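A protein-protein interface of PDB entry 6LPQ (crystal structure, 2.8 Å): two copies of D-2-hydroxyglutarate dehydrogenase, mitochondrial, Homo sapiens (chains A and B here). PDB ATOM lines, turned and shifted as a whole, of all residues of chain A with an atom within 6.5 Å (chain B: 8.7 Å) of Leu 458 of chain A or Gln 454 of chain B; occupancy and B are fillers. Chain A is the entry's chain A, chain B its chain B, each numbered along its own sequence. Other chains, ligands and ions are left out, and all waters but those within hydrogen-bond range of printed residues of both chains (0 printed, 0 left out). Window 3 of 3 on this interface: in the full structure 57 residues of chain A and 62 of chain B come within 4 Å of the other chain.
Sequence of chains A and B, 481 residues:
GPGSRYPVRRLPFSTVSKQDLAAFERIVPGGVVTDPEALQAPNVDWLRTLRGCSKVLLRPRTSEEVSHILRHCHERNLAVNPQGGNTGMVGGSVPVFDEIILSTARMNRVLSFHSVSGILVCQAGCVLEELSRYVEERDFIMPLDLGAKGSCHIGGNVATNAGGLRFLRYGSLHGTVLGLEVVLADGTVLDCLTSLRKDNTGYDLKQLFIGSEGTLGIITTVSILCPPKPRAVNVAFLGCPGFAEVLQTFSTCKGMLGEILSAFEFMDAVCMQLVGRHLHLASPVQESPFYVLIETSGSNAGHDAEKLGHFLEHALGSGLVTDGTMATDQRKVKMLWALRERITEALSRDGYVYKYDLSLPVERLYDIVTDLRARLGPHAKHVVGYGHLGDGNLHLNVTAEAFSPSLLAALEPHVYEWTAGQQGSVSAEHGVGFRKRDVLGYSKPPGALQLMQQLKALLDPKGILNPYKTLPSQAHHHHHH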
ATOM      1  N   GLN A 453      34.182   9.803  -9.759  1.00  0.00           N
ATOM      2  CA  GLN A 453      35.326  10.700  -9.909  1.00  0.00           C
ATOM      3  C   GLN A 453      35.525  11.140 -11.356  1.00  0.00           C
ATOM      4  O   GLN A 453      35.895  12.291 -11.610  1.00  0.00           O
ATOM      5  CB  GLN A 453      36.594  10.033  -9.374  1.00  0.00           C
ATOM      6  CG  GLN A 453      37.815  10.952  -9.316  1.00  0.00           C
ATOM      7  CD  GLN A 453      37.593  12.216  -8.502  1.00  0.00           C
ATOM      8  OE1 GLN A 453      37.078  12.171  -7.386  1.00  0.00           O
ATOM      9  NE2 GLN A 453      37.991  13.355  -9.064  1.00  0.00           N
ATOM     10  N   GLN A 454      35.282  10.246 -12.318  1.00  0.00           N
ATOM     11  CA  GLN A 454      35.369  10.649 -13.719  1.00  0.00           C
ATOM     12  C   GLN A 454      34.305  11.681 -14.073  1.00  0.00           C
ATOM     13  O   GLN A 454      34.573  12.617 -14.838  1.00  0.00           O
ATOM     14  CB  GLN A 454      35.245   9.428 -14.631  1.00  0.00           C
ATOM     15  CG  GLN A 454      36.383   8.429 -14.511  1.00  0.00           C
ATOM     16  CD  GLN A 454      36.159   7.196 -15.366  1.00  0.00           C
ATOM     17  OE1 GLN A 454      35.788   6.134 -14.865  1.00  0.00           O
ATOM     18  NE2 GLN A 454      36.387   7.332 -16.666  1.00  0.00           N
ATOM     19  N   LEU A 455      33.090  11.525 -13.545  1.00  0.00           N
ATOM     20  CA  LEU A 455      32.061  12.530 -13.791  1.00  0.00           C
ATOM     21  C   LEU A 455      32.425  13.860 -13.141  1.00  0.00           C
ATOM     22  O   LEU A 455      32.237  14.923 -13.744  1.00  0.00           O
ATOM     23  CB  LEU A 455      30.704  12.038 -13.290  1.00  0.00           C
ATOM     24  CG  LEU A 455      30.081  10.899 -14.094  1.00  0.00           C
ATOM     25  CD1 LEU A 455      28.957  10.252 -13.312  1.00  0.00           C
ATOM     26  CD2 LEU A 455      29.580  11.403 -15.435  1.00  0.00           C
ATOM     27  N   LYS A 456      32.923  13.815 -11.902  1.00  0.00           N
ATOM     28  CA  LYS A 456      33.418  15.021 -11.242  1.00  0.00           C
ATOM     29  C   LYS A 456      34.498  15.713 -12.068  1.00  0.00           C
ATOM     30  O   LYS A 456      34.484  16.940 -12.220  1.00  0.00           O
ATOM     31  CB  LYS A 456      33.946  14.663  -9.851  1.00  0.00           C
ATOM     32  CG  LYS A 456      34.651  15.796  -9.119  1.00  0.00           C
ATOM     33  CD  LYS A 456      33.746  17.005  -8.963  1.00  0.00           C
ATOM     34  CE  LYS A 456      34.469  18.147  -8.273  1.00  0.00           C
ATOM     35  NZ  LYS A 456      33.532  19.218  -7.832  1.00  0.00           N
ATOM     36  N   ALA A 457      35.442  14.940 -12.610  1.00  0.00           N
ATOM     37  CA  ALA A 457      36.513  15.508 -13.423  1.00  0.00           C
ATOM     38  C   ALA A 457      35.996  16.110 -14.725  1.00  0.00           C
ATOM     39  O   ALA A 457      36.538  17.114 -15.201  1.00  0.00           O
ATOM     40  CB  ALA A 457      37.565  14.441 -13.722  1.00  0.00           C
ATOM     41  N   LEU A 458      34.963  15.511 -15.317  1.00  0.00           N
ATOM     42  CA  LEU A 458      34.360  16.080 -16.517  1.00  0.00           C
ATOM     43  C   LEU A 458      33.632  17.386 -16.216  1.00  0.00           C
ATOM     44  O   LEU A 458      33.821  18.386 -16.918  1.00  0.00           O
ATOM     45  CB  LEU A 458      33.414  15.063 -17.153  1.00  0.00           C
ATOM     46  CG  LEU A 458      32.527  15.551 -18.298  1.00  0.00           C
ATOM     47  CD1 LEU A 458      33.366  16.145 -19.420  1.00  0.00           C
ATOM     48  CD2 LEU A 458      31.665  14.413 -18.819  1.00  0.00           C
ATOM     49  N   LEU A 459      32.813  17.408 -15.165  1.00  0.00           N
ATOM     50  CA  LEU A 459      31.970  18.575 -14.923  1.00  0.00           C
ATOM     51  C   LEU A 459      32.715  19.699 -14.217  1.00  0.00           C
ATOM     52  O   LEU A 459      32.358  20.872 -14.390  1.00  0.00           O
ATOM     53  CB  LEU A 459      30.722  18.181 -14.134  1.00  0.00           C
ATOM     54  CG  LEU A 459      29.691  17.402 -14.952  1.00  0.00           C
ATOM     55  CD1 LEU A 459      28.638  16.775 -14.051  1.00  0.00           C
ATOM     56  CD2 LEU A 459      29.054  18.312 -15.987  1.00  0.00           C
ATOM     57  N   ASP A 460      33.737  19.380 -13.423  1.00  0.00           N
ATOM     58  CA  ASP A 460      34.461  20.387 -12.646  1.00  0.00           C
ATOM     59  C   ASP A 460      35.921  19.963 -12.578  1.00  0.00           C
ATOM     60  O   ASP A 460      36.424  19.531 -11.534  1.00  0.00           O
ATOM     61  CB  ASP A 460      33.842  20.542 -11.254  1.00  0.00           C
ATOM     62  CG  ASP A 460      34.616  21.495 -10.365  1.00  0.00           C
ATOM     63  OD1 ASP A 460      35.329  22.374 -10.898  1.00  0.00           O
ATOM     64  OD2 ASP A 460      34.491  21.372  -9.128  1.00  0.00           O
ATOM     65  N   PRO A 461      36.631  20.050 -13.708  1.00  0.00           N
ATOM     66  CA  PRO A 461      38.034  19.604 -13.748  1.00  0.00           C
ATOM     67  C   PRO A 461      38.950  20.330 -12.780  1.00  0.00           C
ATOM     68  O   PRO A 461      39.916  19.734 -12.286  1.00  0.00           O
ATOM     69  CB  PRO A 461      38.446  19.869 -15.205  1.00  0.00           C
ATOM     70  CG  PRO A 461      37.426  20.823 -15.737  1.00  0.00           C
ATOM     71  CD  PRO A 461      36.161  20.502 -15.027  1.00  0.00           C
ATOM     72  N   LEU B 208      21.850   7.646 -15.170  1.00  0.00           N
ATOM     73  CA  LEU B 208      22.390   7.892 -16.506  1.00  0.00           C
ATOM     74  C   LEU B 208      21.956   6.845 -17.523  1.00  0.00           C
ATOM     75  O   LEU B 208      21.805   7.160 -18.708  1.00  0.00           O
ATOM     76  CB  LEU B 208      23.916   7.934 -16.468  1.00  0.00           C
ATOM     77  CG  LEU B 208      24.601   9.086 -15.749  1.00  0.00           C
ATOM     78  CD1 LEU B 208      25.206   8.596 -14.446  1.00  0.00           C
ATOM     79  CD2 LEU B 208      25.665   9.694 -16.650  1.00  0.00           C
ATOM     80  N   LEU B 216      25.171   4.315 -23.749  1.00  0.00           N
ATOM     81  CA  LEU B 216      26.132   4.484 -22.671  1.00  0.00           C
ATOM     82  C   LEU B 216      26.535   3.179 -22.005  1.00  0.00           C
ATOM     83  O   LEU B 216      27.516   3.163 -21.254  1.00  0.00           O
ATOM     84  CB  LEU B 216      25.576   5.440 -21.604  1.00  0.00           C
ATOM     85  CG  LEU B 216      25.270   6.864 -22.072  1.00  0.00           C
ATOM     86  CD1 LEU B 216      24.683   7.688 -20.941  1.00  0.00           C
ATOM     87  CD2 LEU B 216      26.516   7.531 -22.628  1.00  0.00           C
ATOM     88  N   PRO B 446      20.826  23.855 -26.917  1.00  0.00           N
ATOM     89  CA  PRO B 446      22.147  23.384 -27.370  1.00  0.00           C
ATOM     90  C   PRO B 446      23.082  22.956 -26.251  1.00  0.00           C
ATOM     91  O   PRO B 446      23.752  21.923 -26.373  1.00  0.00           O
ATOM     92  CB  PRO B 446      22.697  24.594 -28.140  1.00  0.00           C
ATOM     93  CG  PRO B 446      21.481  25.322 -28.609  1.00  0.00           C
ATOM     94  CD  PRO B 446      20.453  25.142 -27.529  1.00  0.00           C
ATOM     95  N   GLY B 447      23.146  23.721 -25.159  1.00  0.00           N
ATOM     96  CA  GLY B 447      24.052  23.374 -24.074  1.00  0.00           C
ATOM     97  C   GLY B 447      23.744  22.031 -23.439  1.00  0.00           C
ATOM     98  O   GLY B 447      24.655  21.285 -23.075  1.00  0.00           O
ATOM     99  N   ALA B 448      22.458  21.709 -23.287  1.00  0.00           N
ATOM    100  CA  ALA B 448      22.074  20.387 -22.799  1.00  0.00           C
ATOM    101  C   ALA B 448      22.521  19.298 -23.769  1.00  0.00           C
ATOM    102  O   ALA B 448      23.075  18.270 -23.359  1.00  0.00           O
ATOM    103  CB  ALA B 448      20.563  20.328 -22.576  1.00  0.00           C
ATOM    104  N   LEU B 449      22.281  19.511 -25.064  1.00  0.00           N
ATOM    105  CA  LEU B 449      22.701  18.562 -26.090  1.00  0.00           C
ATOM    106  C   LEU B 449      24.209  18.338 -26.076  1.00  0.00           C
ATOM    107  O   LEU B 449      24.676  17.229 -26.354  1.00  0.00           O
ATOM    108  CB  LEU B 449      22.260  19.044 -27.471  1.00  0.00           C
ATOM    109  CG  LEU B 449      20.765  19.174 -27.762  1.00  0.00           C
ATOM    110  CD1 LEU B 449      20.557  19.746 -29.154  1.00  0.00           C
ATOM    111  CD2 LEU B 449      20.062  17.837 -27.632  1.00  0.00           C
ATOM    112  N   GLN B 450      24.983  19.377 -25.764  1.00  0.00           N
ATOM    113  CA  GLN B 450      26.433  19.228 -25.701  1.00  0.00           C
ATOM    114  C   GLN B 450      26.861  18.350 -24.529  1.00  0.00           C
ATOM    115  O   GLN B 450      27.726  17.479 -24.684  1.00  0.00           O
ATOM    116  CB  GLN B 450      27.077  20.611 -25.584  1.00  0.00           C
ATOM    117  CG  GLN B 450      28.594  20.628 -25.648  1.00  0.00           C
ATOM    118  CD  GLN B 450      29.170  21.964 -25.208  1.00  0.00           C
ATOM    119  OE1 GLN B 450      29.117  22.957 -25.937  1.00  0.00           O
ATOM    120  NE2 GLN B 450      29.717  21.995 -23.998  1.00  0.00           N
ATOM    121  N   LEU B 451      26.281  18.568 -23.347  1.00  0.00           N
ATOM    122  CA  LEU B 451      26.648  17.753 -22.192  1.00  0.00           C
ATOM    123  C   LEU B 451      26.369  16.268 -22.422  1.00  0.00           C
ATOM    124  O   LEU B 451      27.141  15.411 -21.975  1.00  0.00           O
ATOM    125  CB  LEU B 451      25.921  18.258 -20.946  1.00  0.00           C
ATOM    126  CG  LEU B 451      26.182  17.465 -19.665  1.00  0.00           C
ATOM    127  CD1 LEU B 451      27.676  17.437 -19.367  1.00  0.00           C
ATOM    128  CD2 LEU B 451      25.415  18.074 -18.506  1.00  0.00           C
ATOM    129  N   MET B 452      25.282  15.939 -23.130  1.00  0.00           N
ATOM    130  CA  MET B 452      25.022  14.542 -23.479  1.00  0.00           C
ATOM    131  C   MET B 452      26.132  13.961 -24.347  1.00  0.00           C
ATOM    132  O   MET B 452      26.538  12.808 -24.158  1.00  0.00           O
ATOM    133  CB  MET B 452      23.662  14.393 -24.161  1.00  0.00           C
ATOM    134  CG  MET B 452      22.492  14.665 -23.227  1.00  0.00           C
ATOM    135  SD  MET B 452      20.871  14.714 -24.016  1.00  0.00           S
ATOM    136  CE  MET B 452      21.317  15.196 -25.674  1.00  0.00           C
ATOM    137  N   GLN B 453      26.627  14.737 -25.311  1.00  0.00           N
ATOM    138  CA  GLN B 453      27.724  14.273 -26.154  1.00  0.00           C
ATOM    139  C   GLN B 453      28.998  14.051 -25.345  1.00  0.00           C
ATOM    140  O   GLN B 453      29.742  13.097 -25.598  1.00  0.00           O
ATOM    141  CB  GLN B 453      27.961  15.260 -27.295  1.00  0.00           C
ATOM    142  CG  GLN B 453      26.756  15.405 -28.212  1.00  0.00           C
ATOM    143  CD  GLN B 453      26.967  16.420 -29.317  1.00  0.00           C
ATOM    144  OE1 GLN B 453      28.094  16.835 -29.589  1.00  0.00           O
ATOM    145  NE2 GLN B 453      25.878  16.823 -29.966  1.00  0.00           N
ATOM    146  N   GLN B 454      29.267  14.919 -24.367  1.00  0.00           N
ATOM    147  CA  GLN B 454      30.431  14.722 -23.508  1.00  0.00           C
ATOM    148  C   GLN B 454      30.298  13.456 -22.669  1.00  0.00           C
ATOM    149  O   GLN B 454      31.282  12.739 -22.459  1.00  0.00           O
ATOM    150  CB  GLN B 454      30.614  15.933 -22.595  1.00  0.00           C
ATOM    151  CG  GLN B 454      30.966  17.225 -23.302  1.00  0.00           C
ATOM    152  CD  GLN B 454      30.914  18.414 -22.364  1.00  0.00           C
ATOM    153  OE1 GLN B 454      29.931  19.155 -22.339  1.00  0.00           O
ATOM    154  NE2 GLN B 454      31.964  18.590 -21.570  1.00  0.00           N
ATOM    155  N   LEU B 455      29.093  13.169 -22.175  1.00  0.00           N
ATOM    156  CA  LEU B 455      28.860  11.914 -21.467  1.00  0.00           C
ATOM    157  C   LEU B 455      29.129  10.708 -22.363  1.00  0.00           C
ATOM    158  O   LEU B 455      29.774   9.742 -21.938  1.00  0.00           O
ATOM    159  CB  LEU B 455      27.432  11.877 -20.924  1.00  0.00           C
ATOM    160  CG  LEU B 455      27.168  12.811 -19.742  1.00  0.00           C
ATOM    161  CD1 LEU B 455      25.720  12.712 -19.293  1.00  0.00           C
ATOM    162  CD2 LEU B 455      28.121  12.529 -18.590  1.00  0.00           C
ATOM    163  N   LYS B 456      28.639  10.753 -23.605  1.00  0.00           N
ATOM    164  CA  LYS B 456      28.885   9.677 -24.562  1.00  0.00           C
ATOM    165  C   LYS B 456      30.377   9.463 -24.792  1.00  0.00           C
ATOM    166  O   LYS B 456      30.860   8.325 -24.798  1.00  0.00           O
ATOM    167  CB  LYS B 456      28.181  10.008 -25.882  1.00  0.00           C
ATOM    168  CG  LYS B 456      28.427   9.045 -27.038  1.00  0.00           C
ATOM    169  CD  LYS B 456      27.931   7.638 -26.755  1.00  0.00           C
ATOM    170  CE  LYS B 456      28.255   6.712 -27.919  1.00  0.00           C
ATOM    171  NZ  LYS B 456      27.643   5.366 -27.769  1.00  0.00           N
ATOM    172  N   ALA B 457      31.121  10.551 -24.995  1.00  0.00           N
ATOM    173  CA  ALA B 457      32.565  10.454 -25.200  1.00  0.00           C
ATOM    174  C   ALA B 457      33.284   9.871 -23.989  1.00  0.00           C
ATOM    175  O   ALA B 457      34.217   9.074 -24.140  1.00  0.00           O
ATOM    176  CB  ALA B 457      33.136  11.830 -25.540  1.00  0.00           C
ATOM    177  N   LEU B 458      32.873  10.260 -22.780  1.00  0.00           N
ATOM    178  CA  LEU B 458      33.454   9.677 -21.571  1.00  0.00           C
ATOM    179  C   LEU B 458      33.184   8.181 -21.465  1.00  0.00           C
ATOM    180  O   LEU B 458      34.099   7.392 -21.204  1.00  0.00           O
ATOM    181  CB  LEU B 458      32.910  10.402 -20.338  1.00  0.00           C
ATOM    182  CG  LEU B 458      33.343   9.888 -18.964  1.00  0.00           C
ATOM    183  CD1 LEU B 458      34.821  10.138 -18.722  1.00  0.00           C
ATOM    184  CD2 LEU B 458      32.504  10.539 -17.874  1.00  0.00           C
ATOM    185  N   LEU B 459      31.938   7.767 -21.675  1.00  0.00           N
ATOM    186  CA  LEU B 459      31.559   6.385 -21.402  1.00  0.00           C
ATOM    187  C   LEU B 459      31.809   5.451 -22.579  1.00  0.00           C
ATOM    188  O   LEU B 459      32.033   4.254 -22.372  1.00  0.00           O
ATOM    189  CB  LEU B 459      30.090   6.318 -20.974  1.00  0.00           C
ATOM    190  CG  LEU B 459      29.849   6.771 -19.528  1.00  0.00           C
ATOM    191  CD1 LEU B 459      28.383   7.070 -19.281  1.00  0.00           C
ATOM    192  CD2 LEU B 459      30.365   5.742 -18.535  1.00  0.00           C
ATOM    193  N   ASP B 460      31.755   5.961 -23.805  1.00  0.00           N
ATOM    194  CA  ASP B 460      31.982   5.163 -25.010  1.00  0.00           C
ATOM    195  C   ASP B 460      32.786   5.997 -25.997  1.00  0.00           C
ATOM    196  O   ASP B 460      32.270   6.449 -27.025  1.00  0.00           O
ATOM    197  CB  ASP B 460      30.647   4.709 -25.604  1.00  0.00           C
ATOM    198  CG  ASP B 460      30.809   3.857 -26.843  1.00  0.00           C
ATOM    199  OD1 ASP B 460      31.918   3.329 -27.078  1.00  0.00           O
ATOM    200  OD2 ASP B 460      29.814   3.715 -27.583  1.00  0.00           O
ATOM    201  N   PRO B 461      34.070   6.233 -25.703  1.00  0.00           N
ATOM    202  CA  PRO B 461      34.881   7.069 -26.607  1.00  0.00           C
ATOM    203  C   PRO B 461      35.026   6.513 -28.013  1.00  0.00           C
ATOM    204  O   PRO B 461      35.199   7.297 -28.955  1.00  0.00           O
ATOM    205  CB  PRO B 461      36.245   7.142 -25.900  1.00  0.00           C
ATOM    206  CG  PRO B 461      36.246   6.041 -24.908  1.00  0.00           C
ATOM    207  CD  PRO B 461      34.827   5.794 -24.519  1.00  0.00           C
ATOM    208  N   LEU B 471      21.795  10.750 -30.054  1.00  0.00           N
ATOM    209  CA  LEU B 471      22.176  12.146 -29.957  1.00  0.00           C
ATOM    210  C   LEU B 471      22.337  12.742 -31.352  1.00  0.00           C
ATOM    211  O   LEU B 471      22.460  12.012 -32.340  1.00  0.00           O
ATOM    212  CB  LEU B 471      23.503  12.252 -29.198  1.00  0.00           C
ATOM    213  CG  LEU B 471      23.543  11.490 -27.875  1.00  0.00           C
ATOM    214  CD1 LEU B 471      24.947  11.505 -27.301  1.00  0.00           C
ATOM    215  CD2 LEU B 471      22.541  12.056 -26.888  1.00  0.00           C
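The side-chain amide nitrogen (NE2) of Gln 450 of chain B is in hydrogen-bond range of the side-chain amide oxygen (OE1) of Gln 454 of chain B, 3.3 Å away.
Among the printed residues, pairs that only touch across the chains: Gln 454 of chain A with Leu 458 of chain B, Leu 455 of chain A with Leu 455 of chain B, Leu 455 of chain A with Leu 458 of chain B, Leu 458 of chain A with Gln 454 of chain B and Leu 459 of chain A with Leu 451 of chain B.
Of chain B, only Gln 454 comes within 4 Å of Leu 458 of chain A. Printed residues of chain A within 4 Å of Leu 451 of chain B: Leu 459. Of the printed residues of chain A, Leu 455 of chain B touches Leu 455 (3.7 Å). Printed residues of chain A within 4 Å of Leu 458 of chain B: Gln 454 and Leu 455. The nearest residue of chain A that does not touch Gln 454 of chain B is Leu 459 of chain A (6.3 Å). The nearest printed residue of chain B that does not touch Gln 454 of chain A is Leu 459 of chain B (6.5 Å).
Printed residues of chain A that touch a printed residue of chain B: Gln 454, Leu 455, Leu 458 and Leu 459. Among the printed residues, no Asp or Glu carboxylate lies within 4 Å of a Lys or Arg side-chain nitrogen of the other chain.
Gln 454 of chain A touches Leu 458 of chain B, and with the chains exchanged Leu 458 of chain A touches Gln 454 of chain B. Leu 455 of chain B touches its own counterpart, Leu 455 of chain A. Leu 455 of chain A touches Leu 458 of chain B, but with the chains exchanged Leu 458 of chain A does not touch Leu 455 of chain B (4.02 Å). Positions printed for both chains: 453, 454, 455, 456, 457, 458, 459, 460 and 461.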
